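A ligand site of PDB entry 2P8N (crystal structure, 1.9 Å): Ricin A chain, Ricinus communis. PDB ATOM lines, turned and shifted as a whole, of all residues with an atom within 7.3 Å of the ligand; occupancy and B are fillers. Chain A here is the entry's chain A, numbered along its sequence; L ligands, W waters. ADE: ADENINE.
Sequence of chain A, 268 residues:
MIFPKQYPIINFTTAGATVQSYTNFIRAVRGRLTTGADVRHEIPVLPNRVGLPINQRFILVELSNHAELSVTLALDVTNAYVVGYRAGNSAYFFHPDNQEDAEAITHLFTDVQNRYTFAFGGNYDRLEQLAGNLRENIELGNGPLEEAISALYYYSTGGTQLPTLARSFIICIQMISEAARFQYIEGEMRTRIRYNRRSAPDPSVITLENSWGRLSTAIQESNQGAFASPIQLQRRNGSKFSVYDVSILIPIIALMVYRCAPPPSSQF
NH1 of Arg 181 lies within hydrogen-bond range of N3 of the ligand (3.0 Å). A nitrogen (N6) of the ligand lies within hydrogen-bond range of the backbone carbonyl oxygen of Gly 122 (3.2 Å). A nitrogen (N1) of the ligand lies within hydrogen-bond range of the backbone NH (N) of Val 82, 2.8 Å away. O of Val 82 lies within hydrogen-bond range of N6 of the ligand, 3.1 Å away.
Residues that only touch the ligand: Tyr 81 (3.3 Å), Ile 173 (3.4 Å), Tyr 124 (3.6 Å), Asn 123 (3.7 Å), Ser 177 (3.8 Å), Ala 80 (3.8 Å) and Phe 94 (3.96 Å).
The backbone NH (N) of Glu 178 sits at hydrogen-bond distance from the backbone carbonyl oxygen (O) of Ile 173 (3.0 Å). NH2 of Arg 181 sits at hydrogen-bond distance from O of Asn 79, 2.7 Å away. OD1 of Asn 79 lies close to N of Tyr 81 (3.0 Å). OE1 of Glu 178 lies within salt-bridge range of NH1 of Arg 181 (3.0 Å). The backbone NH (N) of Phe 94 is in hydrogen-bond range of the backbone carbonyl oxygen (O) of Val 83 (3.0 Å). OH of Tyr 124 lies within hydrogen-bond range of OE2 of Glu 178, at 2.8 Å. The side-chain amide oxygen of Asn 123 lies close to the backbone NH of Asp 125, 3.5 Å away. The side-chain hydroxyl of Tyr 81 lies within hydrogen-bond range of the backbone NH of Asn 123, 3.5 Å away.
Water W1 lies within hydrogen-bond range of OE2 of Glu 178, N9 of the ligand and O of Glu 209.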
ATOM      1  N   ALA A  74     -18.409  26.694  -6.144  1.00  0.00           N
ATOM      2  CA  ALA A  74     -19.641  27.394  -5.834  1.00  0.00           C
ATOM      3  C   ALA A  74     -20.635  27.111  -6.956  1.00  0.00           C
ATOM      4  O   ALA A  74     -20.335  27.342  -8.126  1.00  0.00           O
ATOM      5  CB  ALA A  74     -19.385  28.894  -5.728  1.00  0.00           C
ATOM      6  N   LEU A  75     -21.799  26.602  -6.602  1.00  0.00           N
ATOM      7  CA  LEU A  75     -22.826  26.304  -7.580  1.00  0.00           C
ATOM      8  C   LEU A  75     -24.048  27.190  -7.384  1.00  0.00           C
ATOM      9  O   LEU A  75     -24.458  27.457  -6.252  1.00  0.00           O
ATOM     10  CB  LEU A  75     -23.256  24.830  -7.501  1.00  0.00           C
ATOM     11  CG  LEU A  75     -22.344  23.755  -8.089  1.00  0.00           C
ATOM     12  CD1 LEU A  75     -21.066  23.595  -7.264  1.00  0.00           C
ATOM     13  CD2 LEU A  75     -23.114  22.443  -8.112  1.00  0.00           C
ATOM     14  N   ASN A  79     -29.492  26.723 -11.549  1.00  0.00           N
ATOM     15  CA  ASN A  79     -29.116  25.906 -12.694  1.00  0.00           C
ATOM     16  C   ASN A  79     -28.024  24.859 -12.426  1.00  0.00           C
ATOM     17  O   ASN A  79     -27.585  24.170 -13.338  1.00  0.00           O
ATOM     18  CB  ASN A  79     -28.683  26.803 -13.859  1.00  0.00           C
ATOM     19  CG  ASN A  79     -27.628  27.814 -13.447  1.00  0.00           C
ATOM     20  OD1 ASN A  79     -26.944  27.635 -12.441  1.00  0.00           O
ATOM     21  ND2 ASN A  79     -27.494  28.879 -14.230  1.00  0.00           N
ATOM     22  N   ALA A  80     -27.591  24.750 -11.169  1.00  0.00           N
ATOM     23  CA  ALA A  80     -26.545  23.798 -10.778  1.00  0.00           C
ATOM     24  C   ALA A  80     -25.214  24.145 -11.458  1.00  0.00           C
ATOM     25  O   ALA A  80     -24.280  23.338 -11.495  1.00  0.00           O
ATOM     26  CB  ALA A  80     -26.977  22.382 -11.130  1.00  0.00           C
ATOM     27  N   TYR A  81     -25.123  25.360 -11.980  1.00  0.00           N
ATOM     28  CA  TYR A  81     -23.936  25.813 -12.676  1.00  0.00           C
ATOM     29  C   TYR A  81     -22.777  26.162 -11.722  1.00  0.00           C
ATOM     30  O   TYR A  81     -22.964  26.877 -10.742  1.00  0.00           O
ATOM     31  CB  TYR A  81     -24.334  27.032 -13.535  1.00  0.00           C
ATOM     32  CG  TYR A  81     -23.308  27.535 -14.517  1.00  0.00           C
ATOM     33  CD1 TYR A  81     -22.255  28.352 -14.094  1.00  0.00           C
ATOM     34  CD2 TYR A  81     -23.409  27.243 -15.880  1.00  0.00           C
ATOM     35  CE1 TYR A  81     -21.331  28.864 -14.998  1.00  0.00           C
ATOM     36  CE2 TYR A  81     -22.486  27.761 -16.797  1.00  0.00           C
ATOM     37  CZ  TYR A  81     -21.450  28.563 -16.348  1.00  0.00           C
ATOM     38  OH  TYR A  81     -20.536  29.077 -17.243  1.00  0.00           O
ATOM     39  N   VAL A  82     -21.595  25.615 -12.008  1.00  0.00           N
ATOM     40  CA  VAL A  82     -20.409  25.916 -11.217  1.00  0.00           C
ATOM     41  C   VAL A  82     -20.006  27.318 -11.655  1.00  0.00           C
ATOM     42  O   VAL A  82     -19.680  27.518 -12.834  1.00  0.00           O
ATOM     43  CB  VAL A  82     -19.238  24.955 -11.546  1.00  0.00           C
ATOM     44  CG1 VAL A  82     -17.970  25.442 -10.855  1.00  0.00           C
ATOM     45  CG2 VAL A  82     -19.577  23.538 -11.099  1.00  0.00           C
ATOM     46  N   VAL A  83     -20.030  28.281 -10.742  1.00  0.00           N
ATOM     47  CA  VAL A  83     -19.702  29.662 -11.080  1.00  0.00           C
ATOM     48  C   VAL A  83     -18.281  30.108 -10.709  1.00  0.00           C
ATOM     49  O   VAL A  83     -17.832  31.177 -11.124  1.00  0.00           O
ATOM     50  CB  VAL A  83     -20.694  30.642 -10.416  1.00  0.00           C
ATOM     51  CG1 VAL A  83     -22.131  30.272 -10.806  1.00  0.00           C
ATOM     52  CG2 VAL A  83     -20.527  30.618  -8.915  1.00  0.00           C
ATOM     53  N   GLY A  84     -17.598  29.291  -9.927  1.00  0.00           N
ATOM     54  CA  GLY A  84     -16.238  29.635  -9.531  1.00  0.00           C
ATOM     55  C   GLY A  84     -15.761  28.720  -8.420  1.00  0.00           C
ATOM     56  O   GLY A  84     -16.462  27.782  -8.037  1.00  0.00           O
ATOM     57  N   PHE A  94     -15.921  32.487 -13.105  1.00  0.00           N
ATOM     58  CA  PHE A  94     -16.066  32.556 -14.557  1.00  0.00           C
ATOM     59  C   PHE A  94     -16.682  33.921 -14.882  1.00  0.00           C
ATOM     60  O   PHE A  94     -17.286  34.559 -14.012  1.00  0.00           O
ATOM     61  CB  PHE A  94     -16.992  31.451 -15.055  1.00  0.00           C
ATOM     62  CG  PHE A  94     -16.407  30.063 -14.936  1.00  0.00           C
ATOM     63  CD1 PHE A  94     -15.216  29.734 -15.586  1.00  0.00           C
ATOM     64  CD2 PHE A  94     -17.050  29.089 -14.182  1.00  0.00           C
ATOM     65  CE1 PHE A  94     -14.681  28.439 -15.485  1.00  0.00           C
ATOM     66  CE2 PHE A  94     -16.524  27.795 -14.071  1.00  0.00           C
ATOM     67  CZ  PHE A  94     -15.336  27.475 -14.725  1.00  0.00           C
ATOM     68  N   GLY A 121     -16.003  32.664 -20.170  1.00  0.00           N
ATOM     69  CA  GLY A 121     -17.141  32.011 -19.533  1.00  0.00           C
ATOM     70  C   GLY A 121     -16.844  30.566 -19.161  1.00  0.00           C
ATOM     71  O   GLY A 121     -15.809  30.026 -19.543  1.00  0.00           O
ATOM     72  N   GLY A 122     -17.760  29.937 -18.414  1.00  0.00           N
ATOM     73  CA  GLY A 122     -17.558  28.565 -18.000  1.00  0.00           C
ATOM     74  C   GLY A 122     -18.322  27.530 -18.817  1.00  0.00           C
ATOM     75  O   GLY A 122     -18.494  26.398 -18.375  1.00  0.00           O
ATOM     76  N   ASN A 123     -18.768  27.918 -20.001  1.00  0.00           N
ATOM     77  CA  ASN A 123     -19.508  27.011 -20.867  1.00  0.00           C
ATOM     78  C   ASN A 123     -18.553  26.019 -21.518  1.00  0.00           C
ATOM     79  O   ASN A 123     -17.374  26.319 -21.714  1.00  0.00           O
ATOM     80  CB  ASN A 123     -20.276  27.806 -21.934  1.00  0.00           C
ATOM     81  CG  ASN A 123     -19.367  28.718 -22.737  1.00  0.00           C
ATOM     82  OD1 ASN A 123     -18.695  28.287 -23.674  1.00  0.00           O
ATOM     83  ND2 ASN A 123     -19.325  29.996 -22.362  1.00  0.00           N
ATOM     84  N   TYR A 124     -19.050  24.827 -21.853  1.00  0.00           N
ATOM     85  CA  TYR A 124     -18.202  23.815 -22.469  1.00  0.00           C
ATOM     86  C   TYR A 124     -17.483  24.287 -23.723  1.00  0.00           C
ATOM     87  O   TYR A 124     -16.291  24.016 -23.901  1.00  0.00           O
ATOM     88  CB  TYR A 124     -19.013  22.562 -22.818  1.00  0.00           C
ATOM     89  CG  TYR A 124     -19.476  21.770 -21.620  1.00  0.00           C
ATOM     90  CD1 TYR A 124     -18.608  21.498 -20.557  1.00  0.00           C
ATOM     91  CD2 TYR A 124     -20.771  21.263 -21.552  1.00  0.00           C
ATOM     92  CE1 TYR A 124     -19.030  20.742 -19.457  1.00  0.00           C
ATOM     93  CE2 TYR A 124     -21.202  20.500 -20.461  1.00  0.00           C
ATOM     94  CZ  TYR A 124     -20.328  20.245 -19.416  1.00  0.00           C
ATOM     95  OH  TYR A 124     -20.752  19.496 -18.351  1.00  0.00           O
ATOM     96  N   ASP A 125     -18.188  24.995 -24.603  1.00  0.00           N
ATOM     97  CA  ASP A 125     -17.541  25.474 -25.830  1.00  0.00           C
ATOM     98  C   ASP A 125     -16.213  26.174 -25.542  1.00  0.00           C
ATOM     99  O   ASP A 125     -15.196  25.849 -26.148  1.00  0.00           O
ATOM    100  CB  ASP A 125     -18.453  26.420 -26.609  1.00  0.00           C
ATOM    101  CG  ASP A 125     -19.729  25.750 -27.068  1.00  0.00           C
ATOM    102  OD1 ASP A 125     -19.677  24.557 -27.472  1.00  0.00           O
ATOM    103  OD2 ASP A 125     -20.789  26.414 -27.047  1.00  0.00           O
ATOM    104  N   LEU A 127     -14.441  26.226 -22.551  1.00  0.00           N
ATOM    105  CA  LEU A 127     -13.545  25.364 -21.773  1.00  0.00           C
ATOM    106  C   LEU A 127     -12.820  24.368 -22.670  1.00  0.00           C
ATOM    107  O   LEU A 127     -11.630  24.103 -22.474  1.00  0.00           O
ATOM    108  CB  LEU A 127     -14.349  24.630 -20.690  1.00  0.00           C
ATOM    109  CG  LEU A 127     -14.219  25.097 -19.232  1.00  0.00           C
ATOM    110  CD1 LEU A 127     -13.984  26.595 -19.148  1.00  0.00           C
ATOM    111  CD2 LEU A 127     -15.488  24.705 -18.478  1.00  0.00           C
ATOM    112  N   ARG A 135     -15.014  17.162 -24.758  1.00  0.00           N
ATOM    113  CA  ARG A 135     -15.436  16.301 -23.671  1.00  0.00           C
ATOM    114  C   ARG A 135     -15.245  14.831 -24.046  1.00  0.00           C
ATOM    115  O   ARG A 135     -14.787  14.021 -23.236  1.00  0.00           O
ATOM    116  CB  ARG A 135     -16.907  16.566 -23.333  1.00  0.00           C
ATOM    117  CG  ARG A 135     -17.151  17.804 -22.495  1.00  0.00           C
ATOM    118  CD  ARG A 135     -18.634  18.140 -22.443  1.00  0.00           C
ATOM    119  NE  ARG A 135     -19.060  18.837 -23.659  1.00  0.00           N
ATOM    120  CZ  ARG A 135     -20.318  18.953 -24.058  1.00  0.00           C
ATOM    121  NH1 ARG A 135     -21.294  18.420 -23.341  1.00  0.00           N
ATOM    122  NH2 ARG A 135     -20.595  19.633 -25.174  1.00  0.00           N
ATOM    123  N   PHE A 169     -11.768  21.758 -14.953  1.00  0.00           N
ATOM    124  CA  PHE A 169     -13.110  22.275 -14.739  1.00  0.00           C
ATOM    125  C   PHE A 169     -14.085  21.340 -15.444  1.00  0.00           C
ATOM    126  O   PHE A 169     -15.144  20.994 -14.902  1.00  0.00           O
ATOM    127  CB  PHE A 169     -13.291  23.675 -15.314  1.00  0.00           C
ATOM    128  CG  PHE A 169     -12.683  24.780 -14.488  1.00  0.00           C
ATOM    129  CD1 PHE A 169     -12.870  24.830 -13.110  1.00  0.00           C
ATOM    130  CD2 PHE A 169     -11.965  25.805 -15.097  1.00  0.00           C
ATOM    131  CE1 PHE A 169     -12.356  25.886 -12.356  1.00  0.00           C
ATOM    132  CE2 PHE A 169     -11.452  26.867 -14.356  1.00  0.00           C
ATOM    133  CZ  PHE A 169     -11.647  26.903 -12.984  1.00  0.00           C
ATOM    134  N   ILE A 173     -17.164  19.714 -13.367  1.00  0.00           N
ATOM    135  CA  ILE A 173     -18.515  20.038 -13.798  1.00  0.00           C
ATOM    136  C   ILE A 173     -19.328  18.795 -14.150  1.00  0.00           C
ATOM    137  O   ILE A 173     -20.481  18.650 -13.744  1.00  0.00           O
ATOM    138  CB  ILE A 173     -18.491  20.984 -15.013  1.00  0.00           C
ATOM    139  CG1 ILE A 173     -17.936  22.354 -14.594  1.00  0.00           C
ATOM    140  CG2 ILE A 173     -19.904  21.144 -15.576  1.00  0.00           C
ATOM    141  CD1 ILE A 173     -17.555  23.260 -15.765  1.00  0.00           C
ATOM    142  N   GLN A 174     -18.740  17.888 -14.917  1.00  0.00           N
ATOM    143  CA  GLN A 174     -19.471  16.691 -15.305  1.00  0.00           C
ATOM    144  C   GLN A 174     -19.718  15.726 -14.158  1.00  0.00           C
ATOM    145  O   GLN A 174     -20.804  15.150 -14.043  1.00  0.00           O
ATOM    146  CB  GLN A 174     -18.758  15.980 -16.443  1.00  0.00           C
ATOM    147  CG  GLN A 174     -18.794  16.750 -17.764  1.00  0.00           C
ATOM    148  CD  GLN A 174     -18.066  16.014 -18.891  1.00  0.00           C
ATOM    149  OE1 GLN A 174     -16.834  16.112 -19.018  1.00  0.00           O
ATOM    150  NE2 GLN A 174     -18.807  15.275 -19.694  1.00  0.00           N
ATOM    151  N   SER A 177     -21.955  18.647 -11.304  1.00  0.00           N
ATOM    152  CA  SER A 177     -23.175  19.274 -11.813  1.00  0.00           C
ATOM    153  C   SER A 177     -23.998  18.364 -12.726  1.00  0.00           C
ATOM    154  O   SER A 177     -25.201  18.190 -12.504  1.00  0.00           O
ATOM    155  CB  SER A 177     -22.832  20.580 -12.540  1.00  0.00           C
ATOM    156  OG  SER A 177     -22.344  21.533 -11.619  1.00  0.00           O
ATOM    157  N   GLU A 178     -23.378  17.780 -13.745  1.00  0.00           N
ATOM    158  CA  GLU A 178     -24.137  16.909 -14.648  1.00  0.00           C
ATOM    159  C   GLU A 178     -24.656  15.668 -13.912  1.00  0.00           C
ATOM    160  O   GLU A 178     -25.764  15.199 -14.205  1.00  0.00           O
ATOM    161  CB  GLU A 178     -23.276  16.521 -15.850  1.00  0.00           C
ATOM    162  CG  GLU A 178     -22.783  17.727 -16.660  1.00  0.00           C
ATOM    163  CD  GLU A 178     -23.888  18.464 -17.421  1.00  0.00           C
ATOM    164  OE1 GLU A 178     -25.077  18.279 -17.097  1.00  0.00           O
ATOM    165  OE2 GLU A 178     -23.558  19.245 -18.331  1.00  0.00           O
ATOM    166  N   ARG A 181     -27.754  16.625 -12.035  1.00  0.00           N
ATOM    167  CA  ARG A 181     -28.860  16.829 -12.976  1.00  0.00           C
ATOM    168  C   ARG A 181     -29.453  15.529 -13.531  1.00  0.00           C
ATOM    169  O   ARG A 181     -30.681  15.423 -13.703  1.00  0.00           O
ATOM    170  CB  ARG A 181     -28.408  17.682 -14.155  1.00  0.00           C
ATOM    171  CG  ARG A 181     -28.065  19.126 -13.850  1.00  0.00           C
ATOM    172  CD  ARG A 181     -27.252  19.703 -15.000  1.00  0.00           C
ATOM    173  NE  ARG A 181     -27.053  21.135 -14.870  1.00  0.00           N
ATOM    174  CZ  ARG A 181     -26.037  21.797 -15.420  1.00  0.00           C
ATOM    175  NH1 ARG A 181     -25.121  21.150 -16.121  1.00  0.00           N
ATOM    176  NH2 ARG A 181     -25.937  23.111 -15.260  1.00  0.00           N
ATOM    177  N   GLU A 209     -26.132  15.905 -21.555  1.00  0.00           N
ATOM    178  CA  GLU A 209     -25.585  17.174 -21.054  1.00  0.00           C
ATOM    179  C   GLU A 209     -26.004  18.341 -21.948  1.00  0.00           C
ATOM    180  O   GLU A 209     -26.397  19.405 -21.469  1.00  0.00           O
ATOM    181  CB  GLU A 209     -24.049  17.099 -21.001  1.00  0.00           C
ATOM    182  CG  GLU A 209     -23.494  15.959 -20.165  1.00  0.00           C
ATOM    183  CD  GLU A 209     -21.971  15.941 -20.156  1.00  0.00           C
ATOM    184  OE1 GLU A 209     -21.359  16.479 -21.108  1.00  0.00           O
ATOM    185  OE2 GLU A 209     -21.385  15.378 -19.209  1.00  0.00           O
ATOM    186  N   TRP A 212     -30.157  19.160 -21.649  1.00  0.00           N
ATOM    187  CA  TRP A 212     -30.822  19.493 -20.384  1.00  0.00           C
ATOM    188  C   TRP A 212     -31.800  20.663 -20.458  1.00  0.00           C
ATOM    189  O   TRP A 212     -32.932  20.570 -19.986  1.00  0.00           O
ATOM    190  CB  TRP A 212     -29.769  19.783 -19.305  1.00  0.00           C
ATOM    191  CG  TRP A 212     -30.344  19.885 -17.923  1.00  0.00           C
ATOM    192  CD1 TRP A 212     -31.054  18.928 -17.254  1.00  0.00           C
ATOM    193  CD2 TRP A 212     -30.192  20.987 -17.002  1.00  0.00           C
ATOM    194  NE1 TRP A 212     -31.351  19.365 -15.978  1.00  0.00           N
ATOM    195  CE2 TRP A 212     -30.841  20.616 -15.805  1.00  0.00           C
ATOM    196  CE3 TRP A 212     -29.576  22.242 -17.093  1.00  0.00           C
ATOM    197  CZ2 TRP A 212     -30.888  21.469 -14.689  1.00  0.00           C
ATOM    198  CZ3 TRP A 212     -29.635  23.096 -15.968  1.00  0.00           C
ATOM    199  CH2 TRP A 212     -30.278  22.696 -14.792  1.00  0.00           C
HETATM  200  N9  ADE L   1     -22.126  23.137 -18.236  1.00  0.00           N
HETATM  201  C8  ADE L   1     -21.166  23.863 -18.899  1.00  0.00           C
HETATM  202  N7  ADE L   1     -20.474  24.646 -18.127  1.00  0.00           N
HETATM  203  C5  ADE L   1     -20.980  24.431 -16.887  1.00  0.00           C
HETATM  204  C6  ADE L   1     -20.667  24.976 -15.633  1.00  0.00           C
HETATM  205  N6  ADE L   1     -19.689  25.877 -15.483  1.00  0.00           N
HETATM  206  N1  ADE L   1     -21.414  24.513 -14.589  1.00  0.00           N
HETATM  207  C2  ADE L   1     -22.381  23.605 -14.789  1.00  0.00           C
HETATM  208  N3  ADE L   1     -22.774  23.019 -15.913  1.00  0.00           N
HETATM  209  C4  ADE L   1     -22.011  23.509 -16.925  1.00  0.00           C
HETATM  210  O   HOH W   1     -24.364  21.384 -19.611  1.00  0.00           O
